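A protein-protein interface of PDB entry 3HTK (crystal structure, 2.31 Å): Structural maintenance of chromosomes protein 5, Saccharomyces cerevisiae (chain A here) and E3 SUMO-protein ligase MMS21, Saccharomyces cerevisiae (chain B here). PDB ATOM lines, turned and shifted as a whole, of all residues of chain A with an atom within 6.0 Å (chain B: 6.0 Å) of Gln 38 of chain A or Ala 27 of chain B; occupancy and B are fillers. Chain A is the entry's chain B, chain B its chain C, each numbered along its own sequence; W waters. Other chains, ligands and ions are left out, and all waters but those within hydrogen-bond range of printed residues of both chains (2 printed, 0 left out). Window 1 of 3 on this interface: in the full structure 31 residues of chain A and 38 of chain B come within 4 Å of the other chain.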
ATOM      1  N   SER A  33     -25.054  15.121  26.051  1.00  0.00           N
ATOM      2  CA  SER A  33     -25.690  16.307  25.484  1.00  0.00           C
ATOM      3  C   SER A  33     -24.999  16.706  24.187  1.00  0.00           C
ATOM      4  O   SER A  33     -25.632  17.223  23.266  1.00  0.00           O
ATOM      5  CB  SER A  33     -25.630  17.484  26.454  1.00  0.00           C
ATOM      6  OG  SER A  33     -26.765  17.504  27.298  1.00  0.00           O
ATOM      7  N   LEU A  34     -23.695  16.466  24.135  1.00  0.00           N
ATOM      8  CA  LEU A  34     -22.911  16.800  22.964  1.00  0.00           C
ATOM      9  C   LEU A  34     -23.331  15.871  21.817  1.00  0.00           C
ATOM     10  O   LEU A  34     -23.550  16.330  20.700  1.00  0.00           O
ATOM     11  CB  LEU A  34     -21.411  16.671  23.287  1.00  0.00           C
ATOM     12  CG  LEU A  34     -20.362  17.201  22.298  1.00  0.00           C
ATOM     13  CD1 LEU A  34     -20.340  16.337  21.069  1.00  0.00           C
ATOM     14  CD2 LEU A  34     -20.663  18.645  21.923  1.00  0.00           C
ATOM     15  N   LYS A  35     -23.448  14.577  22.100  1.00  0.00           N
ATOM     16  CA  LYS A  35     -23.876  13.607  21.098  1.00  0.00           C
ATOM     17  C   LYS A  35     -25.240  14.003  20.546  1.00  0.00           C
ATOM     18  O   LYS A  35     -25.496  13.814  19.362  1.00  0.00           O
ATOM     19  CB  LYS A  35     -23.995  12.205  21.690  1.00  0.00           C
ATOM     20  CG  LYS A  35     -22.745  11.689  22.336  1.00  0.00           C
ATOM     21  CD  LYS A  35     -22.998  10.361  23.056  1.00  0.00           C
ATOM     22  CE  LYS A  35     -23.038   9.168  22.099  1.00  0.00           C
ATOM     23  NZ  LYS A  35     -24.254   9.090  21.255  1.00  0.00           N
ATOM     24  N   ASN A  36     -26.118  14.536  21.398  1.00  0.00           N
ATOM     25  CA  ASN A  36     -27.444  14.959  20.948  1.00  0.00           C
ATOM     26  C   ASN A  36     -27.355  16.123  19.985  1.00  0.00           C
ATOM     27  O   ASN A  36     -28.059  16.134  18.987  1.00  0.00           O
ATOM     28  CB  ASN A  36     -28.355  15.357  22.110  1.00  0.00           C
ATOM     29  CG  ASN A  36     -28.823  14.171  22.910  1.00  0.00           C
ATOM     30  OD1 ASN A  36     -29.087  13.104  22.353  1.00  0.00           O
ATOM     31  ND2 ASN A  36     -28.937  14.346  24.231  1.00  0.00           N
ATOM     32  N   CYS A  37     -26.515  17.108  20.294  1.00  0.00           N
ATOM     33  CA  CYS A  37     -26.337  18.255  19.408  1.00  0.00           C
ATOM     34  C   CYS A  37     -25.764  17.769  18.092  1.00  0.00           C
ATOM     35  O   CYS A  37     -26.187  18.218  17.020  1.00  0.00           O
ATOM     36  CB  CYS A  37     -25.359  19.272  19.994  1.00  0.00           C
ATOM     37  SG  CYS A  37     -25.986  20.258  21.341  1.00  0.00           S
ATOM     38  N   GLN A  38     -24.788  16.863  18.176  1.00  0.00           N
ATOM     39  CA  GLN A  38     -24.162  16.347  16.970  1.00  0.00           C
ATOM     40  C   GLN A  38     -25.221  15.650  16.125  1.00  0.00           C
ATOM     41  O   GLN A  38     -25.277  15.839  14.919  1.00  0.00           O
ATOM     42  CB  GLN A  38     -23.025  15.373  17.321  1.00  0.00           C
ATOM     43  CG  GLN A  38     -22.505  14.569  16.138  1.00  0.00           C
ATOM     44  CD  GLN A  38     -22.146  13.134  16.509  1.00  0.00           C
ATOM     45  OE1 GLN A  38     -22.884  12.466  17.231  1.00  0.00           O
ATOM     46  NE2 GLN A  38     -21.025  12.648  15.994  1.00  0.00           N
ATOM     47  N   LYS A  39     -26.071  14.858  16.765  1.00  0.00           N
ATOM     48  CA  LYS A  39     -27.117  14.139  16.052  1.00  0.00           C
ATOM     49  C   LYS A  39     -28.133  15.093  15.412  1.00  0.00           C
ATOM     50  O   LYS A  39     -28.510  14.921  14.255  1.00  0.00           O
ATOM     51  CB  LYS A  39     -27.819  13.171  17.007  1.00  0.00           C
ATOM     52  CG  LYS A  39     -28.815  12.222  16.341  1.00  0.00           C
ATOM     53  CD  LYS A  39     -29.306  11.183  17.333  1.00  0.00           C
ATOM     54  CE  LYS A  39     -30.336  10.241  16.716  1.00  0.00           C
ATOM     55  NZ  LYS A  39     -29.792   9.424  15.592  1.00  0.00           N
ATOM     56  N   GLU A  40     -28.558  16.100  16.164  1.00  0.00           N
ATOM     57  CA  GLU A  40     -29.515  17.089  15.684  1.00  0.00           C
ATOM     58  C   GLU A  40     -28.961  17.950  14.540  1.00  0.00           C
ATOM     59  O   GLU A  40     -29.718  18.402  13.668  1.00  0.00           O
ATOM     60  CB  GLU A  40     -29.941  17.988  16.838  1.00  0.00           C
ATOM     61  CG  GLU A  40     -30.722  17.256  17.916  1.00  0.00           C
ATOM     62  CD  GLU A  40     -30.894  18.080  19.175  1.00  0.00           C
ATOM     63  OE1 GLU A  40     -31.306  19.254  19.062  1.00  0.00           O
ATOM     64  OE2 GLU A  40     -30.623  17.548  20.281  1.00  0.00           O
ATOM     65  N   LEU A  41     -27.650  18.175  14.558  1.00  0.00           N
ATOM     66  CA  LEU A  41     -26.993  18.970  13.532  1.00  0.00           C
ATOM     67  C   LEU A  41     -26.986  18.234  12.201  1.00  0.00           C
ATOM     68  O   LEU A  41     -27.336  18.822  11.174  1.00  0.00           O
ATOM     69  CB  LEU A  41     -25.552  19.292  13.924  1.00  0.00           C
ATOM     70  CG  LEU A  41     -24.763  20.008  12.837  1.00  0.00           C
ATOM     71  CD1 LEU A  41     -25.403  21.384  12.550  1.00  0.00           C
ATOM     72  CD2 LEU A  41     -23.303  20.150  13.286  1.00  0.00           C
ATOM     73  N   ILE A  42     -26.579  16.963  12.212  1.00  0.00           N
ATOM     74  CA  ILE A  42     -26.557  16.179  10.981  1.00  0.00           C
ATOM     75  C   ILE A  42     -27.965  15.994  10.406  1.00  0.00           C
ATOM     76  O   ILE A  42     -28.142  15.982   9.185  1.00  0.00           O
ATOM     77  CB  ILE A  42     -25.884  14.781  11.187  1.00  0.00           C
ATOM     78  CG1 ILE A  42     -25.757  14.055   9.845  1.00  0.00           C
ATOM     79  CG2 ILE A  42     -26.680  13.939  12.137  1.00  0.00           C
ATOM     80  CD1 ILE A  42     -24.862  14.751   8.852  1.00  0.00           C
ATOM     81  N   SER A  43     -28.964  15.866  11.280  1.00  0.00           N
ATOM     82  CA  SER A  43     -30.356  15.712  10.846  1.00  0.00           C
ATOM     83  C   SER A  43     -30.826  16.959  10.112  1.00  0.00           C
ATOM     84  O   SER A  43     -31.352  16.885   9.011  1.00  0.00           O
ATOM     85  CB  SER A  43     -31.290  15.518  12.038  1.00  0.00           C
ATOM     86  OG  SER A  43     -31.148  14.239  12.615  1.00  0.00           O
ATOM     87  N   LEU B  25     -21.599  15.758   4.037  1.00  0.00           N
ATOM     88  CA  LEU B  25     -22.470  15.263   5.102  1.00  0.00           C
ATOM     89  C   LEU B  25     -21.775  14.189   5.940  1.00  0.00           C
ATOM     90  O   LEU B  25     -21.288  13.174   5.424  1.00  0.00           O
ATOM     91  CB  LEU B  25     -23.780  14.713   4.520  1.00  0.00           C
ATOM     92  CG  LEU B  25     -24.692  15.756   3.861  1.00  0.00           C
ATOM     93  CD1 LEU B  25     -25.841  15.083   3.101  1.00  0.00           C
ATOM     94  CD2 LEU B  25     -25.228  16.677   4.927  1.00  0.00           C
ATOM     95  N   HIS B  26     -21.712  14.431   7.243  1.00  0.00           N
ATOM     96  CA  HIS B  26     -21.081  13.495   8.167  1.00  0.00           C
ATOM     97  C   HIS B  26     -21.423  13.942   9.566  1.00  0.00           C
ATOM     98  O   HIS B  26     -21.748  15.113   9.790  1.00  0.00           O
ATOM     99  CB  HIS B  26     -19.550  13.484   7.995  1.00  0.00           C
ATOM    100  CG  HIS B  26     -18.850  14.625   8.671  1.00  0.00           C
ATOM    101  ND1 HIS B  26     -19.296  15.929   8.589  1.00  0.00           N
ATOM    102  CD2 HIS B  26     -17.723  14.661   9.423  1.00  0.00           C
ATOM    103  CE1 HIS B  26     -18.472  16.719   9.260  1.00  0.00           C
ATOM    104  NE2 HIS B  26     -17.510  15.974   9.776  1.00  0.00           N
ATOM    105  N   ALA B  27     -21.383  13.005  10.505  1.00  0.00           N
ATOM    106  CA  ALA B  27     -21.658  13.334  11.888  1.00  0.00           C
ATOM    107  C   ALA B  27     -20.342  13.873  12.430  1.00  0.00           C
ATOM    108  O   ALA B  27     -19.278  13.331  12.160  1.00  0.00           O
ATOM    109  CB  ALA B  27     -22.097  12.090  12.652  1.00  0.00           C
ATOM    110  N   ARG B  28     -20.418  14.957  13.178  1.00  0.00           N
ATOM    111  CA  ARG B  28     -19.240  15.598  13.746  1.00  0.00           C
ATOM    112  C   ARG B  28     -18.339  14.644  14.545  1.00  0.00           C
ATOM    113  O   ARG B  28     -18.789  13.990  15.491  1.00  0.00           O
ATOM    114  CB  ARG B  28     -19.697  16.748  14.634  1.00  0.00           C
ATOM    115  CG  ARG B  28     -18.972  18.044  14.392  1.00  0.00           C
ATOM    116  CD  ARG B  28     -19.392  18.687  13.092  1.00  0.00           C
ATOM    117  NE  ARG B  28     -18.933  20.069  13.056  1.00  0.00           N
ATOM    118  CZ  ARG B  28     -19.222  20.927  12.091  1.00  0.00           C
ATOM    119  NH1 ARG B  28     -19.973  20.543  11.067  1.00  0.00           N
ATOM    120  NH2 ARG B  28     -18.758  22.166  12.153  1.00  0.00           N
ATOM    121  N   ASP B  29     -17.065  14.578  14.168  1.00  0.00           N
ATOM    122  CA  ASP B  29     -16.099  13.706  14.842  1.00  0.00           C
ATOM    123  C   ASP B  29     -16.005  14.034  16.341  1.00  0.00           C
ATOM    124  O   ASP B  29     -15.911  15.196  16.727  1.00  0.00           O
ATOM    125  CB  ASP B  29     -14.713  13.865  14.196  1.00  0.00           C
ATOM    126  CG  ASP B  29     -13.691  12.861  14.725  1.00  0.00           C
ATOM    127  OD1 ASP B  29     -12.479  13.141  14.632  1.00  0.00           O
ATOM    128  OD2 ASP B  29     -14.088  11.787  15.223  1.00  0.00           O
ATOM    129  N   LEU B  30     -16.036  13.006  17.183  1.00  0.00           N
ATOM    130  CA  LEU B  30     -15.927  13.223  18.620  1.00  0.00           C
ATOM    131  C   LEU B  30     -14.742  12.451  19.201  1.00  0.00           C
ATOM    132  O   LEU B  30     -14.526  12.445  20.409  1.00  0.00           O
ATOM    133  CB  LEU B  30     -17.240  12.829  19.314  1.00  0.00           C
ATOM    134  CG  LEU B  30     -18.375  13.817  19.019  1.00  0.00           C
ATOM    135  CD1 LEU B  30     -19.616  13.449  19.780  1.00  0.00           C
ATOM    136  CD2 LEU B  30     -17.931  15.222  19.420  1.00  0.00           C
ATOM    137  N   SER B  80     -21.755   6.258  19.003  1.00  0.00           N
ATOM    138  CA  SER B  80     -21.180   7.218  18.076  1.00  0.00           C
ATOM    139  C   SER B  80     -20.524   6.489  16.931  1.00  0.00           C
ATOM    140  O   SER B  80     -20.759   6.823  15.777  1.00  0.00           O
ATOM    141  CB  SER B  80     -20.154   8.105  18.776  1.00  0.00           C
ATOM    142  OG  SER B  80     -20.794   9.152  19.482  1.00  0.00           O
ATOM    143  N   PHE B  83     -23.067   5.177  14.758  1.00  0.00           N
ATOM    144  CA  PHE B  83     -23.730   6.266  14.043  1.00  0.00           C
ATOM    145  C   PHE B  83     -22.997   6.586  12.747  1.00  0.00           C
ATOM    146  O   PHE B  83     -23.621   6.692  11.693  1.00  0.00           O
ATOM    147  CB  PHE B  83     -23.813   7.504  14.947  1.00  0.00           C
ATOM    148  CG  PHE B  83     -24.802   8.549  14.481  1.00  0.00           C
ATOM    149  CD1 PHE B  83     -26.064   8.183  14.026  1.00  0.00           C
ATOM    150  CD2 PHE B  83     -24.477   9.899  14.537  1.00  0.00           C
ATOM    151  CE1 PHE B  83     -26.982   9.138  13.636  1.00  0.00           C
ATOM    152  CE2 PHE B  83     -25.396  10.879  14.148  1.00  0.00           C
ATOM    153  CZ  PHE B  83     -26.647  10.498  13.698  1.00  0.00           C
ATOM    154  N   ASP B  84     -21.676   6.730  12.824  1.00  0.00           N
ATOM    155  CA  ASP B  84     -20.867   7.009  11.641  1.00  0.00           C
ATOM    156  C   ASP B  84     -21.014   5.899  10.606  1.00  0.00           C
ATOM    157  O   ASP B  84     -21.266   6.163   9.430  1.00  0.00           O
ATOM    158  CB  ASP B  84     -19.403   7.136  12.022  1.00  0.00           C
ATOM    159  CG  ASP B  84     -19.112   8.418  12.740  1.00  0.00           C
ATOM    160  OD1 ASP B  84     -18.108   8.467  13.488  1.00  0.00           O
ATOM    161  OD2 ASP B  84     -19.889   9.380  12.546  1.00  0.00           O
ATOM    162  N   ILE B  87     -24.318   6.231   8.891  1.00  0.00           N
ATOM    163  CA  ILE B  87     -24.379   7.400   8.022  1.00  0.00           C
ATOM    164  C   ILE B  87     -23.641   7.065   6.728  1.00  0.00           C
ATOM    165  O   ILE B  87     -24.205   7.196   5.638  1.00  0.00           O
ATOM    166  CB  ILE B  87     -23.721   8.665   8.668  1.00  0.00           C
ATOM    167  CG1 ILE B  87     -24.499   9.118   9.910  1.00  0.00           C
ATOM    168  CG2 ILE B  87     -23.705   9.792   7.681  1.00  0.00           C
ATOM    169  CD1 ILE B  87     -25.969   9.340   9.673  1.00  0.00           C
HETATM  170  O   HOH W   1     -20.420   9.895  15.853  1.00  0.00           O
HETATM  171  O   HOH W   2     -23.016  16.087  13.502  1.00  0.00           O
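Among the printed residues, pairs that only touch across the chains: Leu 34 of chain A with Leu 30 of chain B (3.1 Å), Ile 42 of chain A with His 26 of chain B (3.3 Å), Lys 39 of chain A with Phe 83 of chain B (3.4 Å), Lys 35 of chain A with Ser 80 of chain B (3.4 Å), Gln 38 of chain A with Ala 27 of chain B (3.6 Å) and Ile 42 of chain A with Phe 83 of chain B (3.8 Å).
O of Lys 39 of chain A is in hydrogen-bond range of OG of Ser 43 of chain A (3.2 Å).
Printed residues of chain A that touch a printed residue of chain B: Leu 34, Lys 35, Gln 38, Lys 39 and Ile 42. Hydrophobic or aromatic side chains of chain A within 4 Å of the printed part of chain B: Leu 34 and Ile 42. Of the 10 printed residues of chain B, 6 touch a printed residue of chain A. Among the printed residues, 7 pairs touch across the chains. Among the printed residues, no Asp or Glu carboxylate lies within 4 Å of a Lys or Arg side-chain nitrogen of the other chain.
The side-chain amide nitrogen of Gln 38 of chain A lies within hydrogen-bond range of the backbone carbonyl oxygen of Arg 28 of chain B.
Water W2 lies within hydrogen-bond range of the backbone carbonyl oxygen of Gln 38 of chain A (2.7 Å) and the backbone NH of Arg 28 of chain B (2.9 Å). Water W1 lies within hydrogen-bond range of the side-chain amide nitrogen of Gln 38 of chain A, the backbone carbonyl oxygen of Ser 80 of chain B and the side-chain carboxylate of Asp 84 of chain B.
Gln 38 of chain A touches just these residues of chain B: Ala 27 (3.6 Å) and Arg 28 (2.7 Å). Printed residues of chain A within 4 Å of His 26 of chain B: Ile 42. Of the printed residues of chain A, Leu 30 of chain B touches Leu 34 (3.1 Å). Printed residues of chain A within 4 Å of Arg 28 of chain B: Gln 38 (2.7 Å). Of the printed residues of chain B, Ile 42 of chain A touches His 26 (3.3 Å) and Phe 83 (3.8 Å). Of the printed residues of chain B, Lys 39 of chain A touches Phe 83. Ser 33 of chain A touches none of the printed residues of chain B. Ser 43 of chain A touches none of the printed residues of chain B. The nearest printed residue of chain B that does not touch Lys 35 of chain A is Leu 30 of chain B (4.4 Å).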
